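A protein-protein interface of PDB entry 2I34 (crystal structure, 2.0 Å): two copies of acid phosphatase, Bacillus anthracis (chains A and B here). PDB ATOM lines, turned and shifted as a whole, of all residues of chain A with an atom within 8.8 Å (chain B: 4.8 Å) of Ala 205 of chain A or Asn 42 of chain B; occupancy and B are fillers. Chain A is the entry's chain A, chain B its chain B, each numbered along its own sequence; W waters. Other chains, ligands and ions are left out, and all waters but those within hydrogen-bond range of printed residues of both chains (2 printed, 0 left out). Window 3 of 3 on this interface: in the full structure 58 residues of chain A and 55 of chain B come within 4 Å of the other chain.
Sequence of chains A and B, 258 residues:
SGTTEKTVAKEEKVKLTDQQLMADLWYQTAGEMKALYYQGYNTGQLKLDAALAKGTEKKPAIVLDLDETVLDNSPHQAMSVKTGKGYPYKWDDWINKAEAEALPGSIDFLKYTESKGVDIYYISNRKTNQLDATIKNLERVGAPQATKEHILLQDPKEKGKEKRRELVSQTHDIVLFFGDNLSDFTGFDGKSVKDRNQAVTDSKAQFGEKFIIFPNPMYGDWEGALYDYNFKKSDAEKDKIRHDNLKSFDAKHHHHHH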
ATOM      1  N   GLN A  39      -9.810 -16.217  11.816  1.00  0.00           N
ATOM      2  CA  GLN A  39     -11.172 -16.662  12.130  1.00  0.00           C
ATOM      3  C   GLN A  39     -11.303 -18.192  12.082  1.00  0.00           C
ATOM      4  O   GLN A  39     -11.902 -18.801  12.986  1.00  0.00           O
ATOM      5  CB  GLN A  39     -12.178 -15.992  11.196  1.00  0.00           C
ATOM      6  CG  GLN A  39     -13.629 -16.467  11.297  1.00  0.00           C
ATOM      7  CD  GLN A  39     -14.594 -15.516  10.620  1.00  0.00           C
ATOM      8  OE1 GLN A  39     -14.914 -14.469  11.164  1.00  0.00           O
ATOM      9  NE2 GLN A  39     -15.017 -15.845   9.406  1.00  0.00           N
ATOM     10  N   THR A  43     -11.802 -20.375  15.470  1.00  0.00           N
ATOM     11  CA  THR A  43     -12.997 -21.200  15.521  1.00  0.00           C
ATOM     12  C   THR A  43     -12.618 -22.652  15.775  1.00  0.00           C
ATOM     13  O   THR A  43     -13.228 -23.319  16.604  1.00  0.00           O
ATOM     14  CB  THR A  43     -13.799 -21.095  14.216  1.00  0.00           C
ATOM     15  OG1 THR A  43     -14.147 -19.726  13.990  1.00  0.00           O
ATOM     16  CG2 THR A  43     -15.065 -21.956  14.288  1.00  0.00           C
ATOM     17  N   LEU A  46     -11.735 -23.186  19.489  1.00  0.00           N
ATOM     18  CA  LEU A  46     -12.965 -23.231  20.266  1.00  0.00           C
ATOM     19  C   LEU A  46     -13.598 -24.619  20.148  1.00  0.00           C
ATOM     20  O   LEU A  46     -13.981 -25.219  21.143  1.00  0.00           O
ATOM     21  CB  LEU A  46     -13.944 -22.158  19.762  1.00  0.00           C
ATOM     22  CG  LEU A  46     -15.296 -21.975  20.459  1.00  0.00           C
ATOM     23  CD1 LEU A  46     -15.149 -21.196  21.750  1.00  0.00           C
ATOM     24  CD2 LEU A  46     -16.299 -21.245  19.556  1.00  0.00           C
ATOM     25  N   LYS A  47     -13.688 -25.129  18.927  1.00  0.00           N
ATOM     26  CA  LYS A  47     -14.309 -26.437  18.691  1.00  0.00           C
ATOM     27  C   LYS A  47     -13.450 -27.607  19.190  1.00  0.00           C
ATOM     28  O   LYS A  47     -13.988 -28.635  19.580  1.00  0.00           O
ATOM     29  CB  LYS A  47     -14.641 -26.606  17.206  1.00  0.00           C
ATOM     30  CG  LYS A  47     -15.611 -25.568  16.675  1.00  0.00           C
ATOM     31  CD  LYS A  47     -17.048 -25.856  17.098  1.00  0.00           C
ATOM     32  CE  LYS A  47     -17.927 -24.612  17.026  1.00  0.00           C
ATOM     33  NZ  LYS A  47     -19.302 -24.912  17.546  1.00  0.00           N
ATOM     34  N   ALA A 199     -23.925 -30.362  -2.305  1.00  0.00           N
ATOM     35  CA  ALA A 199     -23.336 -31.045  -1.141  1.00  0.00           C
ATOM     36  C   ALA A 199     -22.934 -30.076  -0.018  1.00  0.00           C
ATOM     37  O   ALA A 199     -23.089 -30.383   1.161  1.00  0.00           O
ATOM     38  CB  ALA A 199     -22.145 -31.880  -1.575  1.00  0.00           C
ATOM     39  N   VAL A 200     -22.424 -28.900  -0.385  1.00  0.00           N
ATOM     40  CA  VAL A 200     -22.133 -27.854   0.601  1.00  0.00           C
ATOM     41  C   VAL A 200     -23.416 -27.441   1.332  1.00  0.00           C
ATOM     42  O   VAL A 200     -23.474 -27.461   2.564  1.00  0.00           O
ATOM     43  CB  VAL A 200     -21.434 -26.623  -0.043  1.00  0.00           C
ATOM     44  CG1 VAL A 200     -21.338 -25.446   0.966  1.00  0.00           C
ATOM     45  CG2 VAL A 200     -20.054 -27.000  -0.514  1.00  0.00           C
ATOM     46  N   THR A 201     -24.462 -27.127   0.572  1.00  0.00           N
ATOM     47  CA  THR A 201     -25.760 -26.785   1.151  1.00  0.00           C
ATOM     48  C   THR A 201     -26.287 -27.873   2.081  1.00  0.00           C
ATOM     49  O   THR A 201     -26.741 -27.590   3.196  1.00  0.00           O
ATOM     50  CB  THR A 201     -26.776 -26.541   0.043  1.00  0.00           C
ATOM     51  OG1 THR A 201     -26.280 -25.494  -0.797  1.00  0.00           O
ATOM     52  CG2 THR A 201     -28.142 -26.169   0.602  1.00  0.00           C
ATOM     53  N   ASP A 202     -26.240 -29.108   1.604  1.00  0.00           N
ATOM     54  CA  ASP A 202     -26.679 -30.280   2.375  1.00  0.00           C
ATOM     55  C   ASP A 202     -25.898 -30.467   3.688  1.00  0.00           C
ATOM     56  O   ASP A 202     -26.463 -30.919   4.686  1.00  0.00           O
ATOM     57  CB  ASP A 202     -26.509 -31.540   1.533  1.00  0.00           C
ATOM     58  CG  ASP A 202     -27.495 -31.623   0.365  1.00  0.00           C
ATOM     59  OD1 ASP A 202     -28.379 -30.757   0.218  1.00  0.00           O
ATOM     60  OD2 ASP A 202     -27.381 -32.589  -0.406  1.00  0.00           O
ATOM     61  N   SER A 203     -24.598 -30.157   3.661  1.00  0.00           N
ATOM     62  CA  SER A 203     -23.716 -30.239   4.853  1.00  0.00           C
ATOM     63  C   SER A 203     -23.435 -28.875   5.488  1.00  0.00           C
ATOM     64  O   SER A 203     -22.409 -28.688   6.155  1.00  0.00           O
ATOM     65  CB  SER A 203     -22.388 -30.898   4.485  1.00  0.00           C
ATOM     66  OG  SER A 203     -22.553 -32.296   4.369  1.00  0.00           O
ATOM     67  N   LYS A 204     -24.350 -27.926   5.305  1.00  0.00           N
ATOM     68  CA  LYS A 204     -24.113 -26.539   5.740  1.00  0.00           C
ATOM     69  C   LYS A 204     -23.779 -26.423   7.239  1.00  0.00           C
ATOM     70  O   LYS A 204     -22.987 -25.561   7.642  1.00  0.00           O
ATOM     71  CB  LYS A 204     -25.318 -25.652   5.392  1.00  0.00           C
ATOM     72  CG  LYS A 204     -26.626 -26.015   6.086  1.00  0.00           C
ATOM     73  CD  LYS A 204     -27.793 -25.164   5.551  1.00  0.00           C
ATOM     74  CE  LYS A 204     -29.017 -25.191   6.483  1.00  0.00           C
ATOM     75  NZ  LYS A 204     -29.537 -26.579   6.765  1.00  0.00           N
ATOM     76  N   ALA A 205     -24.364 -27.310   8.051  1.00  0.00           N
ATOM     77  CA  ALA A 205     -24.169 -27.270   9.507  1.00  0.00           C
ATOM     78  C   ALA A 205     -22.763 -27.690   9.951  1.00  0.00           C
ATOM     79  O   ALA A 205     -22.367 -27.404  11.072  1.00  0.00           O
ATOM     80  CB  ALA A 205     -25.217 -28.143  10.200  1.00  0.00           C
ATOM     81  N   GLN A 206     -22.013 -28.353   9.069  1.00  0.00           N
ATOM     82  CA  GLN A 206     -20.691 -28.850   9.425  1.00  0.00           C
ATOM     83  C   GLN A 206     -19.619 -27.767   9.367  1.00  0.00           C
ATOM     84  O   GLN A 206     -18.597 -27.873  10.047  1.00  0.00           O
ATOM     85  CB  GLN A 206     -20.313 -30.026   8.522  1.00  0.00           C
ATOM     86  CG  GLN A 206     -21.324 -31.180   8.576  1.00  0.00           C
ATOM     87  CD  GLN A 206     -21.568 -31.692   9.988  1.00  0.00           C
ATOM     88  OE1 GLN A 206     -20.626 -31.942  10.737  1.00  0.00           O
ATOM     89  NE2 GLN A 206     -22.834 -31.849  10.356  1.00  0.00           N
ATOM     90  N   PHE A 207     -19.850 -26.730   8.565  1.00  0.00           N
ATOM     91  CA  PHE A 207     -18.824 -25.719   8.350  1.00  0.00           C
ATOM     92  C   PHE A 207     -18.730 -24.760   9.519  1.00  0.00           C
ATOM     93  O   PHE A 207     -19.725 -24.134   9.931  1.00  0.00           O
ATOM     94  CB  PHE A 207     -19.040 -25.010   7.019  1.00  0.00           C
ATOM     95  CG  PHE A 207     -18.901 -25.927   5.855  1.00  0.00           C
ATOM     96  CD1 PHE A 207     -17.654 -26.422   5.494  1.00  0.00           C
ATOM     97  CD2 PHE A 207     -20.016 -26.349   5.149  1.00  0.00           C
ATOM     98  CE1 PHE A 207     -17.528 -27.317   4.432  1.00  0.00           C
ATOM     99  CE2 PHE A 207     -19.886 -27.235   4.085  1.00  0.00           C
ATOM    100  CZ  PHE A 207     -18.644 -27.712   3.728  1.00  0.00           C
ATOM    101  N   GLY A 208     -17.516 -24.690  10.064  1.00  0.00           N
ATOM    102  CA  GLY A 208     -17.266 -24.041  11.345  1.00  0.00           C
ATOM    103  C   GLY A 208     -17.554 -24.934  12.549  1.00  0.00           C
ATOM    104  O   GLY A 208     -17.452 -24.482  13.668  1.00  0.00           O
ATOM    105  N   GLU A 209     -17.912 -26.194  12.313  1.00  0.00           N
ATOM    106  CA  GLU A 209     -18.206 -27.130  13.380  1.00  0.00           C
ATOM    107  C   GLU A 209     -17.183 -28.259  13.338  1.00  0.00           C
ATOM    108  O   GLU A 209     -16.332 -28.363  14.221  1.00  0.00           O
ATOM    109  CB  GLU A 209     -19.655 -27.644  13.274  1.00  0.00           C
ATOM    110  CG  GLU A 209     -20.007 -28.788  14.245  1.00  0.00           C
ATOM    111  CD  GLU A 209     -19.992 -28.369  15.718  1.00  0.00           C
ATOM    112  OE1 GLU A 209     -20.309 -27.187  16.026  1.00  0.00           O
ATOM    113  OE2 GLU A 209     -19.684 -29.251  16.568  1.00  0.00           O
ATOM    114  N   LYS A 210     -17.263 -29.079  12.292  1.00  0.00           N
ATOM    115  CA  LYS A 210     -16.336 -30.187  12.059  1.00  0.00           C
ATOM    116  C   LYS A 210     -15.352 -29.878  10.925  1.00  0.00           C
ATOM    117  O   LYS A 210     -14.201 -30.300  10.951  1.00  0.00           O
ATOM    118  CB  LYS A 210     -17.134 -31.446  11.728  1.00  0.00           C
ATOM    119  CG  LYS A 210     -16.352 -32.738  11.878  1.00  0.00           C
ATOM    120  N   PHE A 211     -15.831 -29.159   9.917  1.00  0.00           N
ATOM    121  CA  PHE A 211     -15.043 -28.822   8.769  1.00  0.00           C
ATOM    122  C   PHE A 211     -14.701 -27.347   8.874  1.00  0.00           C
ATOM    123  O   PHE A 211     -15.595 -26.494   8.825  1.00  0.00           O
ATOM    124  CB  PHE A 211     -15.828 -29.072   7.476  1.00  0.00           C
ATOM    125  CG  PHE A 211     -16.321 -30.473   7.289  1.00  0.00           C
ATOM    126  CD1 PHE A 211     -15.700 -31.569   7.900  1.00  0.00           C
ATOM    127  CD2 PHE A 211     -17.424 -30.707   6.463  1.00  0.00           C
ATOM    128  CE1 PHE A 211     -16.182 -32.865   7.693  1.00  0.00           C
ATOM    129  CE2 PHE A 211     -17.902 -32.006   6.240  1.00  0.00           C
ATOM    130  CZ  PHE A 211     -17.289 -33.079   6.856  1.00  0.00           C
ATOM    131  N   ILE A 213     -12.965 -24.312   7.085  1.00  0.00           N
ATOM    132  CA  ILE A 213     -12.630 -23.946   5.703  1.00  0.00           C
ATOM    133  C   ILE A 213     -11.865 -22.625   5.648  1.00  0.00           C
ATOM    134  O   ILE A 213     -12.114 -21.703   6.447  1.00  0.00           O
ATOM    135  CB  ILE A 213     -13.918 -23.955   4.786  1.00  0.00           C
ATOM    136  CG1 ILE A 213     -13.606 -23.544   3.332  1.00  0.00           C
ATOM    137  CG2 ILE A 213     -15.045 -23.103   5.372  1.00  0.00           C
ATOM    138  CD1 ILE A 213     -13.339 -24.690   2.424  1.00  0.00           C
ATOM    139  N   TYR B  38     -21.340 -20.041   5.005  1.00  0.00           N
ATOM    140  CA  TYR B  38     -21.995 -20.866   6.031  1.00  0.00           C
ATOM    141  C   TYR B  38     -21.204 -20.884   7.335  1.00  0.00           C
ATOM    142  O   TYR B  38     -21.775 -20.684   8.408  1.00  0.00           O
ATOM    143  CB  TYR B  38     -22.251 -22.302   5.540  1.00  0.00           C
ATOM    144  CG  TYR B  38     -23.418 -22.450   4.572  1.00  0.00           C
ATOM    145  CD1 TYR B  38     -24.684 -21.940   4.882  1.00  0.00           C
ATOM    146  CD2 TYR B  38     -23.269 -23.152   3.376  1.00  0.00           C
ATOM    147  CE1 TYR B  38     -25.735 -22.085   4.026  1.00  0.00           C
ATOM    148  CE2 TYR B  38     -24.328 -23.305   2.503  1.00  0.00           C
ATOM    149  CZ  TYR B  38     -25.556 -22.764   2.827  1.00  0.00           C
ATOM    150  OH  TYR B  38     -26.624 -22.927   1.978  1.00  0.00           O
ATOM    151  N   GLN B  39     -19.891 -21.091   7.237  1.00  0.00           N
ATOM    152  CA  GLN B  39     -19.009 -21.037   8.392  1.00  0.00           C
ATOM    153  C   GLN B  39     -19.097 -19.698   9.146  1.00  0.00           C
ATOM    154  O   GLN B  39     -19.151 -19.670  10.374  1.00  0.00           O
ATOM    155  CB  GLN B  39     -17.570 -21.293   7.956  1.00  0.00           C
ATOM    156  CG  GLN B  39     -16.530 -21.219   9.080  1.00  0.00           C
ATOM    157  CD  GLN B  39     -15.195 -21.843   8.670  1.00  0.00           C
ATOM    158  OE1 GLN B  39     -15.038 -23.064   8.709  1.00  0.00           O
ATOM    159  NE2 GLN B  39     -14.219 -20.997   8.294  1.00  0.00           N
ATOM    160  N   GLY B  40     -19.109 -18.597   8.400  1.00  0.00           N
ATOM    161  CA  GLY B  40     -19.273 -17.267   8.973  1.00  0.00           C
ATOM    162  C   GLY B  40     -20.561 -17.104   9.752  1.00  0.00           C
ATOM    163  O   GLY B  40     -20.537 -16.703  10.917  1.00  0.00           O
ATOM    164  N   TYR B  41     -21.686 -17.449   9.129  1.00  0.00           N
ATOM    165  CA  TYR B  41     -22.999 -17.321   9.791  1.00  0.00           C
ATOM    166  C   TYR B  41     -23.247 -18.358  10.898  1.00  0.00           C
ATOM    167  O   TYR B  41     -23.905 -18.046  11.911  1.00  0.00           O
ATOM    168  CB  TYR B  41     -24.130 -17.275   8.744  1.00  0.00           C
ATOM    169  CG  TYR B  41     -24.154 -15.936   8.043  1.00  0.00           C
ATOM    170  CD1 TYR B  41     -24.471 -14.781   8.750  1.00  0.00           C
ATOM    171  CD2 TYR B  41     -23.805 -15.807   6.696  1.00  0.00           C
ATOM    172  CE1 TYR B  41     -24.460 -13.535   8.145  1.00  0.00           C
ATOM    173  CE2 TYR B  41     -23.800 -14.563   6.075  1.00  0.00           C
ATOM    174  CZ  TYR B  41     -24.121 -13.429   6.807  1.00  0.00           C
ATOM    175  OH  TYR B  41     -24.148 -12.186   6.206  1.00  0.00           O
ATOM    176  N   ASN B  42     -22.701 -19.568  10.739  1.00  0.00           N
ATOM    177  CA  ASN B  42     -22.782 -20.578  11.786  1.00  0.00           C
ATOM    178  C   ASN B  42     -22.075 -20.099  13.043  1.00  0.00           C
ATOM    179  O   ASN B  42     -22.590 -20.227  14.163  1.00  0.00           O
ATOM    180  CB  ASN B  42     -22.177 -21.921  11.327  1.00  0.00           C
ATOM    181  CG  ASN B  42     -23.061 -22.666  10.335  1.00  0.00           C
ATOM    182  OD1 ASN B  42     -24.219 -22.319  10.145  1.00  0.00           O
ATOM    183  ND2 ASN B  42     -22.507 -23.710   9.704  1.00  0.00           N
ATOM    184  N   THR B  43     -20.890 -19.542  12.844  1.00  0.00           N
ATOM    185  CA  THR B  43     -20.121 -18.950  13.926  1.00  0.00           C
ATOM    186  C   THR B  43     -20.829 -17.722  14.531  1.00  0.00           C
ATOM    187  O   THR B  43     -20.856 -17.553  15.757  1.00  0.00           O
ATOM    188  CB  THR B  43     -18.699 -18.593  13.417  1.00  0.00           C
ATOM    189  OG1 THR B  43     -18.109 -19.763  12.815  1.00  0.00           O
ATOM    190  CG2 THR B  43     -17.823 -18.092  14.549  1.00  0.00           C
ATOM    191  N   GLY B  44     -21.401 -16.881  13.676  1.00  0.00           N
ATOM    192  CA  GLY B  44     -22.205 -15.747  14.124  1.00  0.00           C
ATOM    193  C   GLY B  44     -23.322 -16.152  15.076  1.00  0.00           C
ATOM    194  O   GLY B  44     -23.503 -15.543  16.114  1.00  0.00           O
ATOM    195  N   GLN B  45     -24.073 -17.190  14.728  1.00  0.00           N
ATOM    196  CA  GLN B  45     -25.144 -17.684  15.592  1.00  0.00           C
ATOM    197  C   GLN B  45     -24.622 -18.213  16.935  1.00  0.00           C
ATOM    198  O   GLN B  45     -25.181 -17.910  17.990  1.00  0.00           O
ATOM    199  CB  GLN B  45     -25.915 -18.765  14.852  1.00  0.00           C
ATOM    200  CG  GLN B  45     -27.108 -19.324  15.595  1.00  0.00           C
ATOM    201  CD  GLN B  45     -28.112 -19.925  14.652  1.00  0.00           C
ATOM    202  OE1 GLN B  45     -28.405 -19.363  13.563  1.00  0.00           O
ATOM    203  NE2 GLN B  45     -28.650 -21.056  15.041  1.00  0.00           N
ATOM    204  N   LEU B  46     -23.541 -18.992  16.896  1.00  0.00           N
ATOM    205  CA  LEU B  46     -22.910 -19.476  18.128  1.00  0.00           C
ATOM    206  C   LEU B  46     -22.507 -18.314  19.012  1.00  0.00           C
ATOM    207  O   LEU B  46     -22.742 -18.335  20.219  1.00  0.00           O
ATOM    208  CB  LEU B  46     -21.682 -20.334  17.815  1.00  0.00           C
ATOM    209  CG  LEU B  46     -20.870 -20.871  19.002  1.00  0.00           C
ATOM    210  CD1 LEU B  46     -21.545 -22.068  19.626  1.00  0.00           C
ATOM    211  CD2 LEU B  46     -19.463 -21.237  18.558  1.00  0.00           C
HETATM  212  O   HOH W   1     -14.237 -18.077   7.688  1.00  0.00           O
HETATM  213  O   HOH W   2     -18.670 -22.202  14.161  1.00  0.00           O
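Leu 46 of chain A touches its own counterpart, Leu 46 of chain B.
Positions printed for both chains: 39, 43 and 46.
Of the 12 pairs that touch across the chains among the printed residues, 1 has its exchanged pair printed and touching as well.
Hydrophobic or aromatic side chains of chain A within 4 Å of the printed part of chain B: Leu 46, Val 200 and Ile 213.
Along chain A the printed residues that touch a printed residue of chain B span positions 46 to 213.
Of the 9 printed residues of chain B, 4 touch a printed residue of chain A.
Printed residues of chain B that touch a printed residue of chain A: Tyr 38, Gln 39, Asn 42 and Leu 46.
Hydrophobic or aromatic side chains of chain B that line the printed part of chain A: Tyr 38 and Leu 46.
Among the printed residues, 12 pairs touch across the chains.
Among the printed residues, no Asp or Glu carboxylate lies within 4 Å of a Lys or Arg side-chain nitrogen of the other chain.
Water W2 lies within hydrogen-bond range of the backbone carbonyl oxygen of Gly 208 of chain A (2.6 Å) and the side-chain hydroxyl of Thr 43 of chain B (2.8 Å).
Water W1 bridges the side-chain amide nitrogen of Gln 39 of chain A (2.9 Å) and the side-chain amide nitrogen of Gln 39 of chain B (3.0 Å).
Among the printed residues, merely in contact across the chains: Leu 46 of chain A with Leu 46 of chain B, Lys 47 of chain A with Leu 46 of chain B, Val 200 of chain A with Tyr 38 of chain B, Thr 201 of chain A with Tyr 38 of chain B, Lys 204 of chain A with Tyr 38 of chain B, Ala 205 of chain A with Asn 42 of chain B and Phe 207 of chain A with Gln 39 of chain B.
O of Phe 207 of chain A lies within hydrogen-bond range of ND2 of Asn 42 of chain B, at 2.8 Å.
ND2 of Asn 42 of chain B is in hydrogen-bond range of O of Lys 204 of chain A, 2.8 Å away.
The backbone NH of Gly 208 of chain A is in hydrogen-bond range of the side-chain amide oxygen of Gln 39 of chain B, at 3.3 Å.
The backbone carbonyl oxygen (O) of Ile 213 of chain A sits at hydrogen-bond distance from the side-chain amide nitrogen (NE2) of Gln 39 of chain B, 2.9 Å away.
O of Phe 211 of chain A sits close to OE1 of Gln 39 of chain B, at 3.5 Å.
The backbone carbonyl oxygen of Gln 39 of chain B lies within hydrogen-bond range of the side-chain hydroxyl of Thr 43 of chain B, at 2.7 Å.
The side-chain amino group of Lys 47 of chain A lies within salt-bridge range of the side-chain carboxylate of Glu 209 of chain A, at 2.9 Å.
The backbone NH (N) of Phe 211 of chain A lies within hydrogen-bond range of the backbone carbonyl oxygen (O) of Gln 206 of chain A (3.1 Å).
The backbone carbonyl oxygen of Tyr 38 of chain B lies close to the side-chain amide nitrogen of Asn 42 of chain B, 3.4 Å away.
Of the printed residues of chain B, Lys 204 of chain A touches Tyr 38 (3.8 Å) and Asn 42 (2.8 Å).
Of the printed residues of chain B, Phe 207 of chain A touches Gln 39 (3.5 Å) and Asn 42 (2.8 Å).
Printed residues of chain B within 4 Å of Gly 208 of chain A: Gln 39 (3.3 Å).
No residue of chain A comes within 4 Å of Gly 40 of chain B.
Tyr 41 of chain B touches none of the printed residues of chain A.
Of the printed residues of chain A, Asn 42 of chain B touches Lys 204 (2.8 Å), Ala 205 (3.9 Å) and Phe 207 (2.8 Å).
Gly 44 of chain B touches none of the printed residues of chain A.
The nearest printed residue of chain B that does not touch Ala 205 of chain A is Tyr 38 of chain B (6.0 Å).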
